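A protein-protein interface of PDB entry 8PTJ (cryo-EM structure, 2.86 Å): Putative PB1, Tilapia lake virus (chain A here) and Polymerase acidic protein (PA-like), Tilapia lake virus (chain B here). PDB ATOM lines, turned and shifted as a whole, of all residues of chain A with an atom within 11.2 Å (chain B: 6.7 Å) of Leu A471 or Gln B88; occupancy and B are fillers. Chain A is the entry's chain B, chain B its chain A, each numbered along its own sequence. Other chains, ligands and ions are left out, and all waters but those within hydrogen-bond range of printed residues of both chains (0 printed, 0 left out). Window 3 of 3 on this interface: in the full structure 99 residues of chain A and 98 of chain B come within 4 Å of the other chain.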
ATOM      1  N   ASP A 467     -10.500 -14.419   1.344  1.00  0.00           N
ATOM      2  CA  ASP A 467     -10.794 -15.704   0.715  1.00  0.00           C
ATOM      3  C   ASP A 467      -9.869 -15.927  -0.486  1.00  0.00           C
ATOM      4  O   ASP A 467     -10.289 -15.957  -1.644  1.00  0.00           O
ATOM      5  CB  ASP A 467     -12.276 -15.784   0.321  1.00  0.00           C
ATOM      6  CG  ASP A 467     -12.573 -16.923  -0.636  1.00  0.00           C
ATOM      7  OD1 ASP A 467     -11.851 -17.941  -0.596  1.00  0.00           O
ATOM      8  OD2 ASP A 467     -13.533 -16.803  -1.426  1.00  0.00           O
ATOM      9  N   LEU A 468      -8.581 -16.056  -0.184  1.00  0.00           N
ATOM     10  CA  LEU A 468      -7.552 -16.244  -1.193  1.00  0.00           C
ATOM     11  C   LEU A 468      -7.210 -17.721  -1.341  1.00  0.00           C
ATOM     12  O   LEU A 468      -7.436 -18.524  -0.433  1.00  0.00           O
ATOM     13  CB  LEU A 468      -6.291 -15.460  -0.833  1.00  0.00           C
ATOM     14  CG  LEU A 468      -6.445 -13.941  -0.816  1.00  0.00           C
ATOM     15  CD1 LEU A 468      -5.367 -13.305   0.039  1.00  0.00           C
ATOM     16  CD2 LEU A 468      -6.396 -13.398  -2.232  1.00  0.00           C
ATOM     17  N   ASP A 469      -6.659 -18.068  -2.497  1.00  0.00           N
ATOM     18  CA  ASP A 469      -6.259 -19.444  -2.742  1.00  0.00           C
ATOM     19  C   ASP A 469      -5.192 -19.848  -1.729  1.00  0.00           C
ATOM     20  O   ASP A 469      -4.267 -19.067  -1.471  1.00  0.00           O
ATOM     21  CB  ASP A 469      -5.729 -19.599  -4.167  1.00  0.00           C
ATOM     22  CG  ASP A 469      -5.178 -20.984  -4.437  1.00  0.00           C
ATOM     23  OD1 ASP A 469      -5.961 -21.872  -4.837  1.00  0.00           O
ATOM     24  OD2 ASP A 469      -3.961 -21.185  -4.252  1.00  0.00           O
ATOM     25  N   PRO A 470      -5.276 -21.041  -1.133  1.00  0.00           N
ATOM     26  CA  PRO A 470      -4.298 -21.401  -0.093  1.00  0.00           C
ATOM     27  C   PRO A 470      -2.864 -21.442  -0.586  1.00  0.00           C
ATOM     28  O   PRO A 470      -1.944 -21.333   0.232  1.00  0.00           O
ATOM     29  CB  PRO A 470      -4.766 -22.788   0.371  1.00  0.00           C
ATOM     30  CG  PRO A 470      -6.173 -22.904  -0.078  1.00  0.00           C
ATOM     31  CD  PRO A 470      -6.280 -22.101  -1.328  1.00  0.00           C
ATOM     32  N   LEU A 471      -2.638 -21.599  -1.890  1.00  0.00           N
ATOM     33  CA  LEU A 471      -1.287 -21.771  -2.406  1.00  0.00           C
ATOM     34  C   LEU A 471      -0.544 -20.457  -2.610  1.00  0.00           C
ATOM     35  O   LEU A 471       0.681 -20.483  -2.777  1.00  0.00           O
ATOM     36  CB  LEU A 471      -1.326 -22.534  -3.732  1.00  0.00           C
ATOM     37  CG  LEU A 471      -2.125 -23.841  -3.782  1.00  0.00           C
ATOM     38  CD1 LEU A 471      -1.519 -24.781  -4.810  1.00  0.00           C
ATOM     39  CD2 LEU A 471      -2.189 -24.524  -2.422  1.00  0.00           C
ATOM     40  N   VAL A 472      -1.233 -19.320  -2.604  1.00  0.00           N
ATOM     41  CA  VAL A 472      -0.579 -18.035  -2.846  1.00  0.00           C
ATOM     42  C   VAL A 472       0.075 -17.561  -1.552  1.00  0.00           C
ATOM     43  O   VAL A 472      -0.607 -17.448  -0.523  1.00  0.00           O
ATOM     44  CB  VAL A 472      -1.570 -16.992  -3.389  1.00  0.00           C
ATOM     45  CG1 VAL A 472      -2.340 -17.557  -4.573  1.00  0.00           C
ATOM     46  CG2 VAL A 472      -2.522 -16.525  -2.302  1.00  0.00           C
ATOM     47  N   PRO A 473       1.380 -17.296  -1.538  1.00  0.00           N
ATOM     48  CA  PRO A 473       2.001 -16.761  -0.322  1.00  0.00           C
ATOM     49  C   PRO A 473       1.534 -15.344  -0.039  1.00  0.00           C
ATOM     50  O   PRO A 473       1.135 -14.601  -0.939  1.00  0.00           O
ATOM     51  CB  PRO A 473       3.504 -16.799  -0.632  1.00  0.00           C
ATOM     52  CG  PRO A 473       3.648 -17.648  -1.847  1.00  0.00           C
ATOM     53  CD  PRO A 473       2.373 -17.524  -2.601  1.00  0.00           C
ATOM     54  N   HIS A 474       1.591 -14.970   1.238  1.00  0.00           N
ATOM     55  CA  HIS A 474       1.208 -13.626   1.644  1.00  0.00           C
ATOM     56  C   HIS A 474       2.308 -12.601   1.406  1.00  0.00           C
ATOM     57  O   HIS A 474       2.072 -11.406   1.610  1.00  0.00           O
ATOM     58  CB  HIS A 474       0.808 -13.621   3.120  1.00  0.00           C
ATOM     59  CG  HIS A 474      -0.631 -13.960   3.353  1.00  0.00           C
ATOM     60  ND1 HIS A 474      -1.313 -14.878   2.583  1.00  0.00           N
ATOM     61  CD2 HIS A 474      -1.520 -13.501   4.265  1.00  0.00           C
ATOM     62  CE1 HIS A 474      -2.559 -14.972   3.013  1.00  0.00           C
ATOM     63  NE2 HIS A 474      -2.710 -14.146   4.033  1.00  0.00           N
ATOM     64  N   ARG A 475       3.494 -13.033   0.985  1.00  0.00           N
ATOM     65  CA  ARG A 475       4.568 -12.126   0.607  1.00  0.00           C
ATOM     66  C   ARG A 475       4.482 -11.691  -0.849  1.00  0.00           C
ATOM     67  O   ARG A 475       5.321 -10.903  -1.295  1.00  0.00           O
ATOM     68  CB  ARG A 475       5.929 -12.785   0.854  1.00  0.00           C
ATOM     69  CG  ARG A 475       6.164 -13.247   2.281  1.00  0.00           C
ATOM     70  CD  ARG A 475       6.508 -12.083   3.196  1.00  0.00           C
ATOM     71  NE  ARG A 475       7.943 -11.833   3.257  1.00  0.00           N
ATOM     72  CZ  ARG A 475       8.826 -12.645   3.823  1.00  0.00           C
ATOM     73  NH1 ARG A 475       8.458 -13.783   4.387  1.00  0.00           N
ATOM     74  NH2 ARG A 475      10.112 -12.306   3.823  1.00  0.00           N
ATOM     75  N   LEU A 476       3.501 -12.187  -1.597  1.00  0.00           N
ATOM     76  CA  LEU A 476       3.392 -11.854  -3.010  1.00  0.00           C
ATOM     77  C   LEU A 476       3.051 -10.381  -3.192  1.00  0.00           C
ATOM     78  O   LEU A 476       2.210  -9.827  -2.480  1.00  0.00           O
ATOM     79  CB  LEU A 476       2.326 -12.724  -3.675  1.00  0.00           C
ATOM     80  CG  LEU A 476       2.087 -12.481  -5.166  1.00  0.00           C
ATOM     81  CD1 LEU A 476       3.355 -12.736  -5.964  1.00  0.00           C
ATOM     82  CD2 LEU A 476       0.950 -13.353  -5.669  1.00  0.00           C
ATOM     83  N   ILE A 486      -7.940 -10.846  -9.019  1.00  0.00           N
ATOM     84  CA  ILE A 486      -8.115 -11.950  -8.077  1.00  0.00           C
ATOM     85  C   ILE A 486      -9.551 -11.984  -7.570  1.00  0.00           C
ATOM     86  O   ILE A 486     -10.195 -13.042  -7.535  1.00  0.00           O
ATOM     87  CB  ILE A 486      -7.111 -11.826  -6.918  1.00  0.00           C
ATOM     88  CG1 ILE A 486      -5.707 -12.205  -7.388  1.00  0.00           C
ATOM     89  CG2 ILE A 486      -7.532 -12.704  -5.748  1.00  0.00           C
ATOM     90  CD1 ILE A 486      -4.604 -11.658  -6.514  1.00  0.00           C
ATOM     91  N   ARG A 490     -12.256 -15.031  -8.263  1.00  0.00           N
ATOM     92  CA  ARG A 490     -12.844 -15.783  -7.159  1.00  0.00           C
ATOM     93  C   ARG A 490     -14.362 -15.656  -7.156  1.00  0.00           C
ATOM     94  O   ARG A 490     -15.073 -16.646  -6.947  1.00  0.00           O
ATOM     95  CB  ARG A 490     -12.263 -15.311  -5.827  1.00  0.00           C
ATOM     96  CG  ARG A 490     -12.873 -15.993  -4.606  1.00  0.00           C
ATOM     97  CD  ARG A 490     -12.889 -17.508  -4.754  1.00  0.00           C
ATOM     98  NE  ARG A 490     -13.226 -18.183  -3.506  1.00  0.00           N
ATOM     99  CZ  ARG A 490     -13.246 -19.499  -3.351  1.00  0.00           C
ATOM    100  NH1 ARG A 490     -12.960 -20.319  -4.348  1.00  0.00           N
ATOM    101  NH2 ARG A 490     -13.560 -20.006  -2.162  1.00  0.00           N
ATOM    102  N   CYS B  81       6.157 -16.464  -6.050  1.00  0.00           N
ATOM    103  CA  CYS B  81       6.102 -16.111  -7.461  1.00  0.00           C
ATOM    104  C   CYS B  81       4.655 -15.854  -7.846  1.00  0.00           C
ATOM    105  O   CYS B  81       3.737 -16.504  -7.339  1.00  0.00           O
ATOM    106  CB  CYS B  81       6.702 -17.211  -8.341  1.00  0.00           C
ATOM    107  SG  CYS B  81       7.088 -16.678 -10.021  1.00  0.00           S
ATOM    108  N   GLU B  83       3.256 -16.465 -10.740  1.00  0.00           N
ATOM    109  CA  GLU B  83       2.775 -17.648 -11.441  1.00  0.00           C
ATOM    110  C   GLU B  83       2.900 -18.853 -10.519  1.00  0.00           C
ATOM    111  O   GLU B  83       4.012 -19.243 -10.145  1.00  0.00           O
ATOM    112  CB  GLU B  83       3.565 -17.872 -12.729  1.00  0.00           C
ATOM    113  CG  GLU B  83       3.718 -16.629 -13.590  1.00  0.00           C
ATOM    114  CD  GLU B  83       2.395 -16.137 -14.142  1.00  0.00           C
ATOM    115  OE1 GLU B  83       1.550 -16.982 -14.502  1.00  0.00           O
ATOM    116  OE2 GLU B  83       2.201 -14.905 -14.215  1.00  0.00           O
ATOM    117  N   GLN B  84       1.760 -19.445 -10.160  1.00  0.00           N
ATOM    118  CA  GLN B  84       1.770 -20.553  -9.212  1.00  0.00           C
ATOM    119  C   GLN B  84       2.623 -21.708  -9.720  1.00  0.00           C
ATOM    120  O   GLN B  84       3.282 -22.395  -8.931  1.00  0.00           O
ATOM    121  CB  GLN B  84       0.341 -21.024  -8.942  1.00  0.00           C
ATOM    122  CG  GLN B  84      -0.186 -20.634  -7.573  1.00  0.00           C
ATOM    123  CD  GLN B  84       0.303 -21.560  -6.479  1.00  0.00           C
ATOM    124  OE1 GLN B  84       0.079 -22.769  -6.528  1.00  0.00           O
ATOM    125  NE2 GLN B  84       0.977 -20.997  -5.484  1.00  0.00           N
ATOM    126  N   GLU B  85       2.617 -21.944 -11.032  1.00  0.00           N
ATOM    127  CA  GLU B  85       3.378 -23.062 -11.579  1.00  0.00           C
ATOM    128  C   GLU B  85       4.869 -22.889 -11.321  1.00  0.00           C
ATOM    129  O   GLU B  85       5.555 -23.837 -10.922  1.00  0.00           O
ATOM    130  CB  GLU B  85       3.108 -23.199 -13.076  1.00  0.00           C
ATOM    131  CG  GLU B  85       3.989 -24.231 -13.755  1.00  0.00           C
ATOM    132  CD  GLU B  85       3.600 -24.477 -15.193  1.00  0.00           C
ATOM    133  OE1 GLU B  85       4.400 -25.096 -15.922  1.00  0.00           O
ATOM    134  OE2 GLU B  85       2.498 -24.051 -15.596  1.00  0.00           O
ATOM    135  N   TYR B  86       5.393 -21.685 -11.553  1.00  0.00           N
ATOM    136  CA  TYR B  86       6.812 -21.447 -11.309  1.00  0.00           C
ATOM    137  C   TYR B  86       7.138 -21.575  -9.828  1.00  0.00           C
ATOM    138  O   TYR B  86       8.204 -22.081  -9.460  1.00  0.00           O
ATOM    139  CB  TYR B  86       7.214 -20.067 -11.830  1.00  0.00           C
ATOM    140  CG  TYR B  86       6.984 -19.867 -13.312  1.00  0.00           C
ATOM    141  CD1 TYR B  86       6.991 -20.942 -14.191  1.00  0.00           C
ATOM    142  CD2 TYR B  86       6.771 -18.599 -13.834  1.00  0.00           C
ATOM    143  CE1 TYR B  86       6.783 -20.760 -15.544  1.00  0.00           C
ATOM    144  CE2 TYR B  86       6.563 -18.408 -15.185  1.00  0.00           C
ATOM    145  CZ  TYR B  86       6.571 -19.491 -16.035  1.00  0.00           C
ATOM    146  OH  TYR B  86       6.365 -19.306 -17.382  1.00  0.00           O
ATOM    147  N   GLN B  87       6.233 -21.116  -8.961  1.00  0.00           N
ATOM    148  CA  GLN B  87       6.449 -21.265  -7.527  1.00  0.00           C
ATOM    149  C   GLN B  87       6.528 -22.735  -7.134  1.00  0.00           C
ATOM    150  O   GLN B  87       7.410 -23.135  -6.365  1.00  0.00           O
ATOM    151  CB  GLN B  87       5.333 -20.562  -6.758  1.00  0.00           C
ATOM    152  CG  GLN B  87       5.616 -20.384  -5.282  1.00  0.00           C
ATOM    153  CD  GLN B  87       4.379 -20.577  -4.433  1.00  0.00           C
ATOM    154  OE1 GLN B  87       3.459 -19.762  -4.467  1.00  0.00           O
ATOM    155  NE2 GLN B  87       4.348 -21.661  -3.668  1.00  0.00           N
ATOM    156  N   GLN B  88       5.618 -23.558  -7.656  1.00  0.00           N
ATOM    157  CA  GLN B  88       5.665 -24.986  -7.357  1.00  0.00           C
ATOM    158  C   GLN B  88       6.937 -25.617  -7.906  1.00  0.00           C
ATOM    159  O   GLN B  88       7.561 -26.457  -7.244  1.00  0.00           O
ATOM    160  CB  GLN B  88       4.431 -25.680  -7.931  1.00  0.00           C
ATOM    161  CG  GLN B  88       3.122 -25.202  -7.331  1.00  0.00           C
ATOM    162  CD  GLN B  88       2.931 -25.672  -5.904  1.00  0.00           C
ATOM    163  OE1 GLN B  88       3.514 -26.671  -5.485  1.00  0.00           O
ATOM    164  NE2 GLN B  88       2.114 -24.948  -5.147  1.00  0.00           N
ATOM    165  N   ILE B  89       7.338 -25.224  -9.116  1.00  0.00           N
ATOM    166  CA  ILE B  89       8.546 -25.783  -9.717  1.00  0.00           C
ATOM    167  C   ILE B  89       9.761 -25.454  -8.861  1.00  0.00           C
ATOM    168  O   ILE B  89      10.609 -26.313  -8.603  1.00  0.00           O
ATOM    169  CB  ILE B  89       8.718 -25.270 -11.157  1.00  0.00           C
ATOM    170  CG1 ILE B  89       7.652 -25.884 -12.066  1.00  0.00           C
ATOM    171  CG2 ILE B  89      10.113 -25.597 -11.673  1.00  0.00           C
ATOM    172  CD1 ILE B  89       7.566 -25.244 -13.435  1.00  0.00           C
ATOM    173  N   CYS B  90       9.869 -24.202  -8.413  1.00  0.00           N
ATOM    174  CA  CYS B  90      11.022 -23.816  -7.607  1.00  0.00           C
ATOM    175  C   CYS B  90      10.992 -24.498  -6.246  1.00  0.00           C
ATOM    176  O   CYS B  90      12.038 -24.905  -5.728  1.00  0.00           O
ATOM    177  CB  CYS B  90      11.079 -22.296  -7.445  1.00  0.00           C
ATOM    178  SG  CYS B  90       9.771 -21.596  -6.433  1.00  0.00           S
ATOM    179  N   LYS B  91       9.807 -24.634  -5.649  1.00  0.00           N
ATOM    180  CA  LYS B  91       9.707 -25.315  -4.363  1.00  0.00           C
ATOM    181  C   LYS B  91      10.152 -26.766  -4.481  1.00  0.00           C
ATOM    182  O   LYS B  91      10.880 -27.278  -3.623  1.00  0.00           O
ATOM    183  CB  LYS B  91       8.272 -25.234  -3.841  1.00  0.00           C
ATOM    184  CG  LYS B  91       8.079 -25.855  -2.467  1.00  0.00           C
ATOM    185  CD  LYS B  91       6.648 -25.698  -1.988  1.00  0.00           C
ATOM    186  CE  LYS B  91       6.443 -26.337  -0.626  1.00  0.00           C
ATOM    187  NZ  LYS B  91       5.042 -26.189  -0.147  1.00  0.00           N
ATOM    188  N   VAL B  92       9.724 -27.449  -5.543  1.00  0.00           N
ATOM    189  CA  VAL B  92      10.085 -28.852  -5.712  1.00  0.00           C
ATOM    190  C   VAL B  92      11.567 -28.987  -6.042  1.00  0.00           C
ATOM    191  O   VAL B  92      12.259 -29.861  -5.507  1.00  0.00           O
ATOM    192  CB  VAL B  92       9.201 -29.497  -6.795  1.00  0.00           C
ATOM    193  CG1 VAL B  92       9.921 -30.659  -7.468  1.00  0.00           C
ATOM    194  CG2 VAL B  92       7.880 -29.951  -6.200  1.00  0.00           C
ATOM    195  N   GLN B  93      12.074 -28.130  -6.927  1.00  0.00           N
ATOM    196  CA  GLN B  93      13.434 -28.275  -7.429  1.00  0.00           C
ATOM    197  C   GLN B  93      14.477 -27.767  -6.443  1.00  0.00           C
ATOM    198  O   GLN B  93      15.587 -28.307  -6.395  1.00  0.00           O
ATOM    199  CB  GLN B  93      13.570 -27.536  -8.760  1.00  0.00           C
ATOM    200  CG  GLN B  93      14.399 -28.267  -9.792  1.00  0.00           C
ATOM    201  CD  GLN B  93      13.770 -29.572 -10.229  1.00  0.00           C
ATOM    202  OE1 GLN B  93      12.640 -29.883  -9.858  1.00  0.00           O
ATOM    203  NE2 GLN B  93      14.503 -30.344 -11.022  1.00  0.00           N
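Leu A471 touches three residues of chain B.
Of chain A, only Leu A471 comes within 4 Å of Gln B88.
Printed residues of chain A within 4 Å of Gln B87: Leu A471 and Pro A473.
No residue of chain A comes within 4 Å of Lys B91.
No residue of chain A comes within 4 Å of Val B92.
Printed residues of chain B within 4 Å of Pro A473: Gln B87 (3.1 Å).
Of the printed residues of chain B, Leu A476 touches Cys B81.
Of the printed residues of chain A, Gln B84 touches Leu A471 and Val A472.
Of the printed residues of chain B, Val A472 touches Gln B84.
Asp A469 touches none of the printed residues of chain B.
Glu B85 touches none of the printed residues of chain A.
The nearest printed residue of chain B that does not touch Leu A471 is Cys B81 (6.8 Å).
The nearest residue of chain A that does not touch Gln B88 is Val A472 (7.0 Å).
The nearest printed residue of chain B that does not touch Val A472 is Gln B87 (4.7 Å).
The side-chain amide oxygen (OE1) of Gln B84 lies within hydrogen-bond range of the side-chain amide nitrogen (NE2) of Gln B88 (3.3 Å).
NE2 of Gln B84 lies within hydrogen-bond range of OE1 of Gln B87 (3.0 Å).
The backbone carbonyl oxygen (O) of Gln B87 is in hydrogen-bond range of the side-chain sulfur (SG) of Cys B90, 2.8 Å away.
OD2 of Asp A469 is in hydrogen-bond range of N of Leu A471 (2.7 Å).
The side-chain amide nitrogen of Gln B84 lies within hydrogen-bond range of the backbone carbonyl oxygen of Leu A471.
OE1 of Gln B87 sits close to O of Leu A471.
Of the 12 printed residues of chain A, 4 touch a printed residue of chain B.
Hydrophobic or aromatic side chains of chain A within 4 Å of the printed part of chain B: Leu A471, Pro A473 and Leu A476.
Among the printed residues, 6 pairs touch across the chains.
Among the printed residues, pairs that only touch across the chains: Leu A471 with Gln B88 (3.7 Å), Val A472 with Gln B84 (3.999 Å), Pro A473 with Gln B87 (3.1 Å) and Leu A476 with Cys B81 (3.9 Å).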
